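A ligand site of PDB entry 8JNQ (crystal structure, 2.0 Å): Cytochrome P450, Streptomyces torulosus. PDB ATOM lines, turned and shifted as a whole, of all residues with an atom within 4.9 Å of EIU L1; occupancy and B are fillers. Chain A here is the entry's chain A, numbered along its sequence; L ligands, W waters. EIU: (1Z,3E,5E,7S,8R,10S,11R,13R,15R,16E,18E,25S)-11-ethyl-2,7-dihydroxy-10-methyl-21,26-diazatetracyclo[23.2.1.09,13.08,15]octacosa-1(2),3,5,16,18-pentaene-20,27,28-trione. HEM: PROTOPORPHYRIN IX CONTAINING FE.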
ATOM      1  N   ARG A  74     -32.466  -3.949   5.175  1.00  0.00           N
ATOM      2  CA  ARG A  74     -31.896  -2.608   5.051  1.00  0.00           C
ATOM      3  C   ARG A  74     -32.788  -1.706   4.209  1.00  0.00           C
ATOM      4  O   ARG A  74     -33.578  -2.188   3.397  1.00  0.00           O
ATOM      5  CB  ARG A  74     -30.513  -2.653   4.421  1.00  0.00           C
ATOM      6  CG  ARG A  74     -29.513  -3.524   5.152  1.00  0.00           C
ATOM      7  CD  ARG A  74     -28.495  -4.016   4.165  1.00  0.00           C
ATOM      8  NE  ARG A  74     -27.258  -4.453   4.799  1.00  0.00           N
ATOM      9  CZ  ARG A  74     -26.278  -5.033   4.142  1.00  0.00           C
ATOM     10  NH1 ARG A  74     -26.364  -5.291   2.836  1.00  0.00           N
ATOM     11  NH2 ARG A  74     -25.168  -5.370   4.793  1.00  0.00           N
ATOM     12  N   VAL A  76     -32.445   0.247   1.561  1.00  0.00           N
ATOM     13  CA  VAL A  76     -32.315   0.382   0.120  1.00  0.00           C
ATOM     14  C   VAL A  76     -32.309  -1.016  -0.512  1.00  0.00           C
ATOM     15  O   VAL A  76     -31.505  -1.875  -0.121  1.00  0.00           O
ATOM     16  CB  VAL A  76     -31.049   1.172  -0.257  1.00  0.00           C
ATOM     17  CG1 VAL A  76     -30.894   1.249  -1.789  1.00  0.00           C
ATOM     18  CG2 VAL A  76     -31.101   2.590   0.396  1.00  0.00           C
ATOM     19  N   ARG A  78     -31.622  -4.060  -2.940  1.00  0.00           N
ATOM     20  CA  ARG A  78     -30.324  -4.461  -3.448  1.00  0.00           C
ATOM     21  C   ARG A  78     -30.311  -4.411  -4.967  1.00  0.00           C
ATOM     22  O   ARG A  78     -31.327  -4.652  -5.626  1.00  0.00           O
ATOM     23  CB  ARG A  78     -30.001  -5.859  -2.913  1.00  0.00           C
ATOM     24  CG  ARG A  78     -29.176  -6.720  -3.813  1.00  0.00           C
ATOM     25  CD  ARG A  78     -29.026  -8.085  -3.163  1.00  0.00           C
ATOM     26  NE  ARG A  78     -30.179  -8.935  -3.407  1.00  0.00           N
ATOM     27  CZ  ARG A  78     -30.199  -9.876  -4.337  1.00  0.00           C
ATOM     28  NH1 ARG A  78     -29.141 -10.097  -5.105  1.00  0.00           N
ATOM     29  NH2 ARG A  78     -31.301 -10.610  -4.509  1.00  0.00           N
ATOM     30  N   THR A  79     -29.149  -4.067  -5.528  1.00  0.00           N
ATOM     31  CA  THR A  79     -28.900  -4.133  -6.967  1.00  0.00           C
ATOM     32  C   THR A  79     -27.654  -4.965  -7.244  1.00  0.00           C
ATOM     33  O   THR A  79     -26.953  -5.391  -6.323  1.00  0.00           O
ATOM     34  CB  THR A  79     -28.750  -2.728  -7.576  1.00  0.00           C
ATOM     35  OG1 THR A  79     -27.774  -1.988  -6.829  1.00  0.00           O
ATOM     36  CG2 THR A  79     -30.074  -1.979  -7.534  1.00  0.00           C
ATOM     37  N   PHE A  84     -25.737 -13.572  -6.890  1.00  0.00           N
ATOM     38  CA  PHE A  84     -26.986 -13.440  -6.132  1.00  0.00           C
ATOM     39  C   PHE A  84     -28.080 -12.729  -6.920  1.00  0.00           C
ATOM     40  O   PHE A  84     -29.164 -12.507  -6.373  1.00  0.00           O
ATOM     41  CB  PHE A  84     -26.713 -12.702  -4.821  1.00  0.00           C
ATOM     42  CG  PHE A  84     -25.804 -13.445  -3.875  1.00  0.00           C
ATOM     43  CD1 PHE A  84     -26.262 -14.553  -3.186  1.00  0.00           C
ATOM     44  CD2 PHE A  84     -24.499 -13.036  -3.663  1.00  0.00           C
ATOM     45  CE1 PHE A  84     -25.437 -15.225  -2.285  1.00  0.00           C
ATOM     46  CE2 PHE A  84     -23.677 -13.719  -2.769  1.00  0.00           C
ATOM     47  CZ  PHE A  84     -24.140 -14.811  -2.094  1.00  0.00           C
ATOM     48  N   TRP A 164     -15.145  -3.021   7.145  1.00  0.00           N
ATOM     49  CA  TRP A 164     -16.227  -3.081   6.177  1.00  0.00           C
ATOM     50  C   TRP A 164     -17.138  -4.271   6.442  1.00  0.00           C
ATOM     51  O   TRP A 164     -18.368  -4.149   6.347  1.00  0.00           O
ATOM     52  CB  TRP A 164     -15.628  -3.156   4.764  1.00  0.00           C
ATOM     53  CG  TRP A 164     -16.586  -3.566   3.673  1.00  0.00           C
ATOM     54  CD1 TRP A 164     -16.440  -4.631   2.829  1.00  0.00           C
ATOM     55  CD2 TRP A 164     -17.805  -2.899   3.277  1.00  0.00           C
ATOM     56  NE1 TRP A 164     -17.498  -4.671   1.935  1.00  0.00           N
ATOM     57  CE2 TRP A 164     -18.348  -3.624   2.195  1.00  0.00           C
ATOM     58  CE3 TRP A 164     -18.481  -1.773   3.740  1.00  0.00           C
ATOM     59  CZ2 TRP A 164     -19.538  -3.253   1.563  1.00  0.00           C
ATOM     60  CZ3 TRP A 164     -19.672  -1.402   3.108  1.00  0.00           C
ATOM     61  CH2 TRP A 164     -20.178  -2.140   2.039  1.00  0.00           C
ATOM     62  N   VAL A 168     -21.096  -4.248   7.057  1.00  0.00           N
ATOM     63  CA  VAL A 168     -22.013  -5.080   6.282  1.00  0.00           C
ATOM     64  C   VAL A 168     -22.857  -5.962   7.205  1.00  0.00           C
ATOM     65  O   VAL A 168     -24.057  -6.156   6.966  1.00  0.00           O
ATOM     66  CB  VAL A 168     -21.197  -5.915   5.270  1.00  0.00           C
ATOM     67  CG1 VAL A 168     -22.007  -7.102   4.738  1.00  0.00           C
ATOM     68  CG2 VAL A 168     -20.744  -5.035   4.110  1.00  0.00           C
ATOM     69  N   LEU A 178     -23.531   2.922   5.094  1.00  0.00           N
ATOM     70  CA  LEU A 178     -23.395   1.790   4.184  1.00  0.00           C
ATOM     71  C   LEU A 178     -23.036   2.264   2.783  1.00  0.00           C
ATOM     72  O   LEU A 178     -22.175   1.666   2.117  1.00  0.00           O
ATOM     73  CB  LEU A 178     -24.695   0.990   4.162  1.00  0.00           C
ATOM     74  CG  LEU A 178     -24.590  -0.333   3.433  1.00  0.00           C
ATOM     75  CD1 LEU A 178     -23.750  -1.292   4.241  1.00  0.00           C
ATOM     76  CD2 LEU A 178     -25.975  -0.890   3.211  1.00  0.00           C
ATOM     77  N   ILE A 232     -16.785 -10.541   0.444  1.00  0.00           N
ATOM     78  CA  ILE A 232     -17.718 -10.314   1.538  1.00  0.00           C
ATOM     79  C   ILE A 232     -18.167 -11.651   2.122  1.00  0.00           C
ATOM     80  O   ILE A 232     -18.135 -11.851   3.351  1.00  0.00           O
ATOM     81  CB  ILE A 232     -18.907  -9.450   1.079  1.00  0.00           C
ATOM     82  CG1 ILE A 232     -18.434  -8.043   0.752  1.00  0.00           C
ATOM     83  CG2 ILE A 232     -19.994  -9.390   2.161  1.00  0.00           C
ATOM     84  CD1 ILE A 232     -19.545  -7.125   0.253  1.00  0.00           C
ATOM     85  N   ALA A 233     -18.588 -12.589   1.261  1.00  0.00           N
ATOM     86  CA  ALA A 233     -18.964 -13.916   1.752  1.00  0.00           C
ATOM     87  C   ALA A 233     -17.853 -14.518   2.603  1.00  0.00           C
ATOM     88  O   ALA A 233     -18.092 -15.020   3.710  1.00  0.00           O
ATOM     89  CB  ALA A 233     -19.299 -14.842   0.565  1.00  0.00           C
ATOM     90  N   VAL A 236     -17.864 -12.655   6.150  1.00  0.00           N
ATOM     91  CA  VAL A 236     -18.958 -12.611   7.118  1.00  0.00           C
ATOM     92  C   VAL A 236     -19.428 -13.988   7.578  1.00  0.00           C
ATOM     93  O   VAL A 236     -20.205 -14.076   8.550  1.00  0.00           O
ATOM     94  CB  VAL A 236     -20.157 -11.811   6.561  1.00  0.00           C
ATOM     95  CG1 VAL A 236     -19.693 -10.439   6.083  1.00  0.00           C
ATOM     96  CG2 VAL A 236     -20.780 -12.575   5.396  1.00  0.00           C
ATOM     97  N   SER A 237     -18.977 -15.060   6.937  1.00  0.00           N
ATOM     98  CA  SER A 237     -19.607 -16.354   7.168  1.00  0.00           C
ATOM     99  C   SER A 237     -18.843 -17.169   8.204  1.00  0.00           C
ATOM    100  O   SER A 237     -19.264 -17.281   9.366  1.00  0.00           O
ATOM    101  CB  SER A 237     -19.726 -17.097   5.838  1.00  0.00           C
ATOM    102  OG  SER A 237     -18.449 -17.278   5.214  1.00  0.00           O
ATOM    103  N   LEU A 279     -27.976 -19.750  11.904  1.00  0.00           N
ATOM    104  CA  LEU A 279     -26.936 -18.789  11.547  1.00  0.00           C
ATOM    105  C   LEU A 279     -27.480 -17.527  10.906  1.00  0.00           C
ATOM    106  O   LEU A 279     -27.048 -16.432  11.253  1.00  0.00           O
ATOM    107  CB  LEU A 279     -25.930 -19.431  10.593  1.00  0.00           C
ATOM    108  CG  LEU A 279     -24.740 -18.594  10.099  1.00  0.00           C
ATOM    109  CD1 LEU A 279     -23.667 -18.486  11.198  1.00  0.00           C
ATOM    110  CD2 LEU A 279     -24.167 -19.224   8.853  1.00  0.00           C
ATOM    111  N   LEU A 280     -28.409 -17.652   9.969  1.00  0.00           N
ATOM    112  CA  LEU A 280     -28.749 -16.571   9.035  1.00  0.00           C
ATOM    113  C   LEU A 280     -29.975 -15.847   9.562  1.00  0.00           C
ATOM    114  O   LEU A 280     -31.113 -16.187   9.232  1.00  0.00           O
ATOM    115  CB  LEU A 280     -29.007 -17.118   7.646  1.00  0.00           C
ATOM    116  CG  LEU A 280     -27.839 -17.842   7.018  1.00  0.00           C
ATOM    117  CD1 LEU A 280     -28.260 -18.537   5.712  1.00  0.00           C
ATOM    118  CD2 LEU A 280     -26.711 -16.847   6.764  1.00  0.00           C
ATOM    119  N   PHE A 283     -29.445 -12.427   6.330  1.00  0.00           N
ATOM    120  CA  PHE A 283     -28.972 -12.533   4.946  1.00  0.00           C
ATOM    121  C   PHE A 283     -29.786 -13.515   4.078  1.00  0.00           C
ATOM    122  O   PHE A 283     -29.210 -14.255   3.274  1.00  0.00           O
ATOM    123  CB  PHE A 283     -27.503 -12.943   4.949  1.00  0.00           C
ATOM    124  CG  PHE A 283     -26.536 -11.778   5.140  1.00  0.00           C
ATOM    125  CD1 PHE A 283     -26.809 -10.540   4.599  1.00  0.00           C
ATOM    126  CD2 PHE A 283     -25.319 -11.978   5.783  1.00  0.00           C
ATOM    127  CE1 PHE A 283     -25.918  -9.491   4.737  1.00  0.00           C
ATOM    128  CE2 PHE A 283     -24.426 -10.917   5.928  1.00  0.00           C
ATOM    129  CZ  PHE A 283     -24.728  -9.680   5.397  1.00  0.00           C
ATOM    130  N   ASN A 284     -31.106 -13.586   4.239  1.00  0.00           N
ATOM    131  CA  ASN A 284     -31.927 -14.562   3.502  1.00  0.00           C
ATOM    132  C   ASN A 284     -32.542 -13.889   2.290  1.00  0.00           C
ATOM    133  O   ASN A 284     -33.516 -13.145   2.422  1.00  0.00           O
ATOM    134  CB  ASN A 284     -33.016 -15.128   4.413  1.00  0.00           C
ATOM    135  CG  ASN A 284     -32.452 -15.989   5.507  1.00  0.00           C
ATOM    136  OD1 ASN A 284     -31.831 -17.019   5.233  1.00  0.00           O
ATOM    137  ND2 ASN A 284     -32.640 -15.553   6.761  1.00  0.00           N
ATOM    138  N   LEU A 285     -32.011 -14.160   1.105  1.00  0.00           N
ATOM    139  CA  LEU A 285     -32.507 -13.501  -0.100  1.00  0.00           C
ATOM    140  C   LEU A 285     -33.872 -14.053  -0.504  1.00  0.00           C
ATOM    141  O   LEU A 285     -34.029 -15.263  -0.695  1.00  0.00           O
ATOM    142  CB  LEU A 285     -31.527 -13.665  -1.259  1.00  0.00           C
ATOM    143  CG  LEU A 285     -30.183 -13.024  -0.959  1.00  0.00           C
ATOM    144  CD1 LEU A 285     -29.213 -13.278  -2.101  1.00  0.00           C
ATOM    145  CD2 LEU A 285     -30.395 -11.571  -0.750  1.00  0.00           C
ATOM    146  N   VAL A 386     -25.781 -12.130  10.639  1.00  0.00           N
ATOM    147  CA  VAL A 386     -25.304 -13.481  10.869  1.00  0.00           C
ATOM    148  C   VAL A 386     -25.143 -13.633  12.379  1.00  0.00           C
ATOM    149  O   VAL A 386     -24.551 -12.761  13.025  1.00  0.00           O
ATOM    150  CB  VAL A 386     -23.963 -13.728  10.143  1.00  0.00           C
ATOM    151  CG1 VAL A 386     -23.355 -15.068  10.533  1.00  0.00           C
ATOM    152  CG2 VAL A 386     -24.135 -13.663   8.617  1.00  0.00           C
HETATM  153  C1  EIU L   1     -23.883 -12.714   1.225  1.00  0.00           C
HETATM  154  C10 EIU L   1     -23.408 -16.246   5.867  1.00  0.00           C
HETATM  155  C11 EIU L   1     -26.103 -16.514   3.160  1.00  0.00           C
HETATM  156  C12 EIU L   1     -26.355 -13.371   0.886  1.00  0.00           C
HETATM  157  C13 EIU L   1     -26.877 -11.948   1.055  1.00  0.00           C
HETATM  158  C14 EIU L   1     -26.655 -10.958   0.161  1.00  0.00           C
HETATM  159  C15 EIU L   1     -23.995 -11.224   1.542  1.00  0.00           C
HETATM  160  C16 EIU L   1     -23.604 -10.184   0.534  1.00  0.00           C
HETATM  161  C17 EIU L   1     -27.212  -9.572   0.374  1.00  0.00           C
HETATM  162  C18 EIU L   1     -26.850  -8.481  -0.289  1.00  0.00           C
HETATM  163  C19 EIU L   1     -23.729  -8.917   0.926  1.00  0.00           C
HETATM  164  C2  EIU L   1     -25.071 -13.539   1.727  1.00  0.00           C
HETATM  165  C20 EIU L   1     -23.126  -7.859   0.343  1.00  0.00           C
HETATM  166  C21 EIU L   1     -27.388  -7.147  -0.091  1.00  0.00           C
HETATM  167  C24 EIU L   1     -24.258  -3.975  -1.776  1.00  0.00           C
HETATM  168  C25 EIU L   1     -22.927  -4.118   0.370  1.00  0.00           C
HETATM  169  C26 EIU L   1     -24.140  -3.514  -0.316  1.00  0.00           C
HETATM  170  C27 EIU L   1     -27.411  -4.662  -0.472  1.00  0.00           C
HETATM  171  C28 EIU L   1     -26.897  -6.018  -0.710  1.00  0.00           C
HETATM  172  C3  EIU L   1     -22.679 -13.344   1.943  1.00  0.00           C
HETATM  173  C30 EIU L   1     -25.672  -4.468  -2.070  1.00  0.00           C
HETATM  174  C31 EIU L   1     -25.870  -5.949  -1.729  1.00  0.00           C
HETATM  175  C34 EIU L   1     -23.432  -6.479   0.842  1.00  0.00           C
HETATM  176  C4  EIU L   1     -22.958 -14.849   1.751  1.00  0.00           C
HETATM  177  C5  EIU L   1     -24.501 -14.986   1.842  1.00  0.00           C
HETATM  178  C6  EIU L   1     -22.362 -15.708   2.877  1.00  0.00           C
HETATM  179  C7  EIU L   1     -23.550 -16.568   3.312  1.00  0.00           C
HETATM  180  C8  EIU L   1     -24.806 -15.694   3.178  1.00  0.00           C
HETATM  181  C9  EIU L   1     -23.426 -17.228   4.697  1.00  0.00           C
HETATM  182  N23 EIU L   1     -22.799  -5.552   0.109  1.00  0.00           N
HETATM  183  N29 EIU L   1     -26.697  -3.830  -1.261  1.00  0.00           N
HETATM  184  O22 EIU L   1     -28.444  -7.037   0.727  1.00  0.00           O
HETATM  185  O32 EIU L   1     -28.304  -4.334   0.299  1.00  0.00           O
HETATM  186  O33 EIU L   1     -25.256  -6.853  -2.274  1.00  0.00           O
HETATM  187  O35 EIU L   1     -24.164  -6.182   1.794  1.00  0.00           O
HETATM  188  O36 EIU L   1     -27.339 -14.266   1.413  1.00  0.00           O
HETATM  189  CHA HEM L   2     -24.275 -18.982  -1.114  1.00  0.00           C
HETATM  190  CHB HEM L   2     -23.972 -20.511   3.490  1.00  0.00           C
HETATM  191  CHC HEM L   2     -19.174 -19.788   3.449  1.00  0.00           C
HETATM  192  CHD HEM L   2     -19.623 -17.698  -0.906  1.00  0.00           C
HETATM  193  C1A HEM L   2     -24.595 -19.498   0.122  1.00  0.00           C
HETATM  194  C2A HEM L   2     -25.909 -19.934   0.541  1.00  0.00           C
HETATM  195  C3A HEM L   2     -25.821 -20.358   1.800  1.00  0.00           C
HETATM  196  C4A HEM L   2     -24.456 -20.202   2.233  1.00  0.00           C
HETATM  197  CMA HEM L   2     -26.968 -20.910   2.672  1.00  0.00           C
HETATM  198  CAA HEM L   2     -27.196 -19.919  -0.334  1.00  0.00           C
HETATM  199  CBA HEM L   2     -27.918 -18.583  -0.205  1.00  0.00           C
HETATM  200  CGA HEM L   2     -29.212 -18.599  -0.982  1.00  0.00           C
HETATM  201  O1A HEM L   2     -29.954 -17.602  -0.876  1.00  0.00           O
HETATM  202  O2A HEM L   2     -29.497 -19.593  -1.710  1.00  0.00           O
HETATM  203  C1B HEM L   2     -22.669 -20.423   3.886  1.00  0.00           C
HETATM  204  C2B HEM L   2     -22.155 -20.780   5.189  1.00  0.00           C
HETATM  205  C3B HEM L   2     -20.824 -20.565   5.204  1.00  0.00           C
HETATM  206  C4B HEM L   2     -20.447 -20.092   3.884  1.00  0.00           C
HETATM  207  CMB HEM L   2     -23.066 -21.285   6.317  1.00  0.00           C
HETATM  208  CAB HEM L   2     -19.806 -20.810   6.329  1.00  0.00           C
HETATM  209  CBB HEM L   2     -20.109 -21.596   7.359  1.00  0.00           C
HETATM  210  C1C HEM L   2     -18.871 -19.187   2.239  1.00  0.00           C
HETATM  211  C2C HEM L   2     -17.563 -18.787   1.799  1.00  0.00           C
HETATM  212  C3C HEM L   2     -17.695 -18.203   0.589  1.00  0.00           C
HETATM  213  C4C HEM L   2     -19.091 -18.231   0.242  1.00  0.00           C
HETATM  214  CMC HEM L   2     -16.284 -19.038   2.641  1.00  0.00           C
HETATM  215  CAC HEM L   2     -16.649 -17.582  -0.376  1.00  0.00           C
HETATM  216  CBC HEM L   2     -15.345 -17.671  -0.130  1.00  0.00           C
HETATM  217  C1D HEM L   2     -20.920 -17.863  -1.327  1.00  0.00           C
HETATM  218  C2D HEM L   2     -21.437 -17.374  -2.589  1.00  0.00           C
HETATM  219  C3D HEM L   2     -22.728 -17.719  -2.659  1.00  0.00           C
HETATM  220  C4D HEM L   2     -23.052 -18.445  -1.442  1.00  0.00           C
HETATM  221  CMD HEM L   2     -20.594 -16.577  -3.619  1.00  0.00           C
HETATM  222  CAD HEM L   2     -23.683 -17.426  -3.840  1.00  0.00           C
HETATM  223  CBD HEM L   2     -23.585 -18.617  -4.808  1.00  0.00           C
HETATM  224  CGD HEM L   2     -24.478 -18.466  -6.016  1.00  0.00           C
HETATM  225  O1D HEM L   2     -25.496 -17.733  -5.953  1.00  0.00           O
HETATM  226  O2D HEM L   2     -24.166 -19.126  -7.045  1.00  0.00           O
HETATM  227  NA  HEM L   2     -23.721 -19.683   1.182  1.00  0.00           N
HETATM  228  NB  HEM L   2     -21.598 -20.005   3.107  1.00  0.00           N
HETATM  229  NC  HEM L   2     -19.780 -18.844   1.258  1.00  0.00           N
HETATM  230  ND  HEM L   2     -21.930 -18.502  -0.652  1.00  0.00           N
HETATM  231 FE   HEM L   2     -21.682 -19.526   1.114  1.00  0.00          FE
HETATM  232  O   HOH W   1     -29.104  -1.590   0.918  1.00  0.00           O
HETATM  233  O   HOH W   2     -27.252  -0.641  -0.930  1.00  0.00           O
HETATM  234  O   HOH W   3     -29.675 -15.860   1.005  1.00  0.00           O
HETATM  235  O   HOH W   4     -30.972  -8.322   0.998  1.00  0.00           O
HETATM  236  O   HOH W   5     -21.859  -6.417  -2.570  1.00  0.00           O
HETATM  237  O   HOH W   6     -30.790  -4.996   0.793  1.00  0.00           O
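O of Val 168 sits at hydrogen-bond distance from NH2 of Arg 74, 2.6 Å away.
The backbone carbonyl oxygen of Leu 280 lies within hydrogen-bond range of the side-chain amide nitrogen of Asn 284 (3.0 Å).
The backbone carbonyl oxygen (O) of Phe 84 is in hydrogen-bond range of the guanidinium group (NH1) of Arg 78, 2.7 Å away.
O of Ala 233 is in hydrogen-bond range of OG of Ser 237, 2.7 Å away.
CD of Arg 78 touches C21 of EIU L1 (3.6 Å).
Phe 84 touches EIU L1 (CE1 to C12, 3.8 Å).
CZ2 of Trp 164 touches C25 of EIU L1, at 3.7 Å.
Val 168 touches EIU L1 (CG1 to O35, 3.8 Å).
Ile 232 touches EIU L1 (CD1 to N23, 3.6 Å).
CA of Ala 233 touches C3 of EIU L1, at 3.8 Å.
CB of Ser 237 touches C10 of EIU L1, at 3.8 Å.
Leu 280 touches EIU L1 (CD2 to C10, 3.5 Å).
Leu 285 touches EIU L1.
CG2 of Val 386 touches C10 of EIU L1, at 3.8 Å.
12 residues have an atom within 4 Å of EIU L1: Arg 74, Arg 78, Phe 84, Trp 164, Val 168, Ile 232, Ala 233, Ser 237, Leu 280, Phe 283, Leu 285 and Val 386.
The nearest printed residue that does not touch EIU L1 is Val 236 (4.02 Å).
Water W6 lies within hydrogen-bond range of O32 of EIU L1 (2.6 Å) and O of Val 76 (3.3 Å).
Water W3 lies within hydrogen-bond range of an oxygen (O1A) of HEM L2, the backbone carbonyl oxygen (O) of Phe 283, an oxygen (O36) of EIU L1 and the backbone NH (N) of Leu 285.
Water W1 bridges the backbone carbonyl oxygen of Val 76 and an oxygen (O32) of EIU L1.
The guanidinium group (NH1) of Arg 74 lies within hydrogen-bond range of an oxygen (O35) of EIU L1, at 2.6 Å.
O36 of EIU L1 lies within hydrogen-bond range of O of Phe 283, 2.6 Å away.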
